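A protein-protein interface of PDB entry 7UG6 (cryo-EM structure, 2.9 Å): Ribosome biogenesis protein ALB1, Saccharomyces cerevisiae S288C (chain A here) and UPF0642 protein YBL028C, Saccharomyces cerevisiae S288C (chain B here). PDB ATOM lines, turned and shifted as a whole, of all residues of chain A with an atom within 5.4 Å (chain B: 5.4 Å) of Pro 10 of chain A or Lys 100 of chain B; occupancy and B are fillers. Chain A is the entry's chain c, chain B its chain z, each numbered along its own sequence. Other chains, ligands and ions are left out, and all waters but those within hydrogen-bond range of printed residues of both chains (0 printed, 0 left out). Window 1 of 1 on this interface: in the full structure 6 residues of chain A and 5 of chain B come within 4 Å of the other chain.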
ATOM      1  N   ASN A   8       0.886  29.059  18.721  1.00  0.00           N
ATOM      2  CA  ASN A   8      -0.402  28.440  18.457  1.00  0.00           C
ATOM      3  C   ASN A   8      -0.359  27.388  17.356  1.00  0.00           C
ATOM      4  O   ASN A   8      -1.352  26.680  17.175  1.00  0.00           O
ATOM      5  CB  ASN A   8      -1.419  29.518  18.111  1.00  0.00           C
ATOM      6  CG  ASN A   8      -1.858  30.295  19.318  1.00  0.00           C
ATOM      7  OD1 ASN A   8      -2.487  29.754  20.214  1.00  0.00           O
ATOM      8  ND2 ASN A   8      -1.526  31.574  19.352  1.00  0.00           N
ATOM      9  N   ARG A   9       0.744  27.263  16.608  1.00  0.00           N
ATOM     10  CA  ARG A   9       0.894  26.140  15.693  1.00  0.00           C
ATOM     11  C   ARG A   9       1.541  24.978  16.410  1.00  0.00           C
ATOM     12  O   ARG A   9       2.555  25.174  17.094  1.00  0.00           O
ATOM     13  CB  ARG A   9       1.723  26.480  14.461  1.00  0.00           C
ATOM     14  CG  ARG A   9       0.933  26.989  13.293  1.00  0.00           C
ATOM     15  CD  ARG A   9       1.640  26.827  11.943  1.00  0.00           C
ATOM     16  NE  ARG A   9       2.661  27.808  11.608  1.00  0.00           N
ATOM     17  CZ  ARG A   9       3.915  27.792  12.032  1.00  0.00           C
ATOM     18  NH1 ARG A   9       4.359  26.801  12.786  1.00  0.00           N
ATOM     19  NH2 ARG A   9       4.743  28.754  11.650  1.00  0.00           N
ATOM     20  N   PRO A  10       1.003  23.771  16.287  1.00  0.00           N
ATOM     21  CA  PRO A  10       1.786  22.587  16.634  1.00  0.00           C
ATOM     22  C   PRO A  10       2.996  22.504  15.724  1.00  0.00           C
ATOM     23  O   PRO A  10       2.888  22.634  14.506  1.00  0.00           O
ATOM     24  CB  PRO A  10       0.808  21.434  16.401  1.00  0.00           C
ATOM     25  CG  PRO A  10      -0.530  22.058  16.482  1.00  0.00           C
ATOM     26  CD  PRO A  10      -0.365  23.415  15.887  1.00  0.00           C
ATOM     27  N   LYS A  11       4.163  22.322  16.329  1.00  0.00           N
ATOM     28  CA  LYS A  11       5.407  22.200  15.587  1.00  0.00           C
ATOM     29  C   LYS A  11       6.007  20.807  15.724  1.00  0.00           C
ATOM     30  O   LYS A  11       6.317  20.159  14.724  1.00  0.00           O
ATOM     31  CB  LYS A  11       6.403  23.261  16.059  1.00  0.00           C
ATOM     32  CG  LYS A  11       7.606  23.372  15.185  1.00  0.00           C
ATOM     33  CD  LYS A  11       8.502  24.442  15.691  1.00  0.00           C
ATOM     34  CE  LYS A  11       9.588  24.718  14.708  1.00  0.00           C
ATOM     35  NZ  LYS A  11      10.449  25.831  15.157  1.00  0.00           N
ATOM     36  N   LEU A  12       6.197  20.345  16.955  1.00  0.00           N
ATOM     37  CA  LEU A  12       6.683  18.989  17.155  1.00  0.00           C
ATOM     38  C   LEU A  12       5.689  17.963  16.634  1.00  0.00           C
ATOM     39  O   LEU A  12       6.080  16.984  15.990  1.00  0.00           O
ATOM     40  CB  LEU A  12       6.944  18.742  18.634  1.00  0.00           C
ATOM     41  CG  LEU A  12       7.515  17.363  18.933  1.00  0.00           C
ATOM     42  CD1 LEU A  12       8.875  17.192  18.278  1.00  0.00           C
ATOM     43  CD2 LEU A  12       7.566  17.116  20.406  1.00  0.00           C
ATOM     44  N   THR A  13       4.403  18.165  16.917  1.00  0.00           N
ATOM     45  CA  THR A  13       3.390  17.200  16.513  1.00  0.00           C
ATOM     46  C   THR A  13       3.225  17.175  14.999  1.00  0.00           C
ATOM     47  O   THR A  13       3.050  16.107  14.402  1.00  0.00           O
ATOM     48  CB  THR A  13       2.072  17.528  17.206  1.00  0.00           C
ATOM     49  OG1 THR A  13       2.242  17.407  18.622  1.00  0.00           O
ATOM     50  CG2 THR A  13       0.964  16.590  16.748  1.00  0.00           C
ATOM     51  N   SER A  14       3.288  18.343  14.359  1.00  0.00           N
ATOM     52  CA  SER A  14       3.236  18.385  12.904  1.00  0.00           C
ATOM     53  C   SER A  14       4.435  17.680  12.290  1.00  0.00           C
ATOM     54  O   SER A  14       4.294  16.941  11.311  1.00  0.00           O
ATOM     55  CB  SER A  14       3.163  19.829  12.420  1.00  0.00           C
ATOM     56  OG  SER A  14       3.515  19.927  11.049  1.00  0.00           O
ATOM     57  N   HIS A  17       3.878  13.885  12.733  1.00  0.00           N
ATOM     58  CA  HIS A  17       2.899  13.387  11.773  1.00  0.00           C
ATOM     59  C   HIS A  17       3.508  13.295  10.381  1.00  0.00           C
ATOM     60  O   HIS A  17       3.331  12.297   9.670  1.00  0.00           O
ATOM     61  CB  HIS A  17       1.675  14.303  11.765  1.00  0.00           C
ATOM     62  CG  HIS A  17       0.413  13.632  11.322  1.00  0.00           C
ATOM     63  ND1 HIS A  17      -0.191  12.629  12.047  1.00  0.00           N
ATOM     64  CD2 HIS A  17      -0.365  13.829  10.233  1.00  0.00           C
ATOM     65  CE1 HIS A  17      -1.284  12.235  11.421  1.00  0.00           C
ATOM     66  NE2 HIS A  17      -1.411  12.943  10.315  1.00  0.00           N
ATOM     67  N   LYS B  95      -4.675  22.151   3.598  1.00  0.00           N
ATOM     68  CA  LYS B  95      -3.287  21.768   3.842  1.00  0.00           C
ATOM     69  C   LYS B  95      -2.903  21.996   5.295  1.00  0.00           C
ATOM     70  O   LYS B  95      -2.174  21.190   5.881  1.00  0.00           O
ATOM     71  CB  LYS B  95      -2.315  22.525   2.932  1.00  0.00           C
ATOM     72  CG  LYS B  95      -2.432  22.268   1.438  1.00  0.00           C
ATOM     73  CD  LYS B  95      -1.339  23.031   0.679  1.00  0.00           C
ATOM     74  CE  LYS B  95      -1.529  24.541   0.659  1.00  0.00           C
ATOM     75  NZ  LYS B  95      -2.723  24.963  -0.107  1.00  0.00           N
ATOM     76  N   GLN B  96      -3.366  23.097   5.890  1.00  0.00           N
ATOM     77  CA  GLN B  96      -3.042  23.351   7.292  1.00  0.00           C
ATOM     78  C   GLN B  96      -3.750  22.366   8.219  1.00  0.00           C
ATOM     79  O   GLN B  96      -3.197  21.971   9.248  1.00  0.00           O
ATOM     80  CB  GLN B  96      -3.382  24.795   7.650  1.00  0.00           C
ATOM     81  CG  GLN B  96      -2.459  25.790   6.974  1.00  0.00           C
ATOM     82  CD  GLN B  96      -2.654  27.211   7.445  1.00  0.00           C
ATOM     83  OE1 GLN B  96      -3.420  27.473   8.370  1.00  0.00           O
ATOM     84  NE2 GLN B  96      -1.970  28.145   6.796  1.00  0.00           N
ATOM     85  N   SER B  97      -4.967  21.951   7.873  1.00  0.00           N
ATOM     86  CA  SER B  97      -5.667  20.965   8.689  1.00  0.00           C
ATOM     87  C   SER B  97      -5.104  19.561   8.484  1.00  0.00           C
ATOM     88  O   SER B  97      -5.222  18.701   9.365  1.00  0.00           O
ATOM     89  CB  SER B  97      -7.159  20.993   8.373  1.00  0.00           C
ATOM     90  OG  SER B  97      -7.818  19.900   8.983  1.00  0.00           O
ATOM     91  N   LYS B  98      -4.497  19.310   7.328  1.00  0.00           N
ATOM     92  CA  LYS B  98      -3.979  18.007   6.947  1.00  0.00           C
ATOM     93  C   LYS B  98      -2.523  17.804   7.344  1.00  0.00           C
ATOM     94  O   LYS B  98      -2.089  16.658   7.494  1.00  0.00           O
ATOM     95  CB  LYS B  98      -4.220  17.842   5.437  1.00  0.00           C
ATOM     96  CG  LYS B  98      -3.819  16.540   4.769  1.00  0.00           C
ATOM     97  CD  LYS B  98      -2.521  16.733   4.015  1.00  0.00           C
ATOM     98  CE  LYS B  98      -2.741  17.793   2.931  1.00  0.00           C
ATOM     99  NZ  LYS B  98      -1.537  18.184   2.156  1.00  0.00           N
ATOM    100  N   LYS B  99      -1.771  18.881   7.548  1.00  0.00           N
ATOM    101  CA  LYS B  99      -0.442  18.845   8.147  1.00  0.00           C
ATOM    102  C   LYS B  99      -0.421  19.238   9.617  1.00  0.00           C
ATOM    103  O   LYS B  99       0.663  19.255  10.209  1.00  0.00           O
ATOM    104  CB  LYS B  99       0.530  19.739   7.362  1.00  0.00           C
ATOM    105  CG  LYS B  99       0.736  19.331   5.917  1.00  0.00           C
ATOM    106  CD  LYS B  99       1.433  17.978   5.905  1.00  0.00           C
ATOM    107  CE  LYS B  99       1.839  17.542   4.526  1.00  0.00           C
ATOM    108  NZ  LYS B  99       0.685  17.209   3.691  1.00  0.00           N
ATOM    109  N   LYS B 100      -1.580  19.526  10.218  1.00  0.00           N
ATOM    110  CA  LYS B 100      -1.692  19.914  11.629  1.00  0.00           C
ATOM    111  C   LYS B 100      -0.838  21.146  11.930  1.00  0.00           C
ATOM    112  O   LYS B 100      -0.013  21.157  12.844  1.00  0.00           O
ATOM    113  CB  LYS B 100      -1.343  18.747  12.560  1.00  0.00           C
ATOM    114  CG  LYS B 100      -2.377  17.643  12.554  1.00  0.00           C
ATOM    115  CD  LYS B 100      -2.070  16.576  13.574  1.00  0.00           C
ATOM    116  CE  LYS B 100      -3.318  15.788  13.950  1.00  0.00           C
ATOM    117  NZ  LYS B 100      -3.847  14.966  12.824  1.00  0.00           N
ATOM    118  N   THR B 101      -1.044  22.197  11.144  1.00  0.00           N
ATOM    119  CA  THR B 101      -0.258  23.421  11.219  1.00  0.00           C
ATOM    120  C   THR B 101      -1.161  24.642  11.257  1.00  0.00           C
ATOM    121  O   THR B 101      -0.910  25.640  10.578  1.00  0.00           O
ATOM    122  CB  THR B 101       0.710  23.528  10.042  1.00  0.00           C
ATOM    123  OG1 THR B 101      -0.025  23.588   8.813  1.00  0.00           O
ATOM    124  CG2 THR B 101       1.652  22.351  10.002  1.00  0.00           C
ATOM    125  N   SER B 102      -2.234  24.589  12.037  1.00  0.00           N
ATOM    126  CA  SER B 102      -3.202  25.676  12.090  1.00  0.00           C
ATOM    127  C   SER B 102      -3.039  26.494  13.363  1.00  0.00           C
ATOM    128  O   SER B 102      -3.049  25.941  14.468  1.00  0.00           O
ATOM    129  CB  SER B 102      -4.625  25.134  12.002  1.00  0.00           C
ATOM    130  OG  SER B 102      -5.563  26.180  12.164  1.00  0.00           O
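Printed residues of chain B within 4 Å of Asn 8 of chain A: Ser 102. Pro 10 of chain A touches just these residues of chain B: Lys 100 and Ser 102. Printed residues of chain B within 4 Å of Ser 14 of chain A: Lys 99, Lys 100 and Thr 101. Printed residues of chain B within 4 Å of His 17 of chain A: Lys 100. Printed residues of chain A within 4 Å of Lys 100 of chain B: Pro 10, Ser 14 and His 17. Printed residues of chain A within 4 Å of Thr 101 of chain B: Arg 9 (3.1 Å) and Ser 14 (3.2 Å). The nearest printed residue of chain A that does not touch Lys 99 of chain B is His 17 of chain A (5.3 Å).
Thr 101 of chain B touches Arg 9 of chain A (O to CD, 3.1 Å). Pro 10 of chain A touches Lys 100 of chain B (O to O, 3.7 Å). O of Ser 102 of chain B touches CD of Pro 10 of chain A, at 3.9 Å. Ser 14 of chain A touches Lys 100 of chain B. Ser 14 of chain A touches Thr 101 of chain B (OG to CG2, 3.2 Å). NZ of Lys 100 of chain B touches CE1 of His 17 of chain A (3.999 Å).
Among the printed residues, 8 pairs touch across the chains.
The backbone carbonyl oxygen (O) of Asn 8 of chain A lies close to the backbone carbonyl oxygen (O) of Ser 102 of chain B, at 3.3 Å. The backbone carbonyl oxygen of Lys 99 of chain B lies within hydrogen-bond range of the side-chain hydroxyl of Ser 14 of chain A (3.0 Å).
O of Gln 96 of chain B is in hydrogen-bond range of N of Thr 101 of chain B (2.9 Å).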
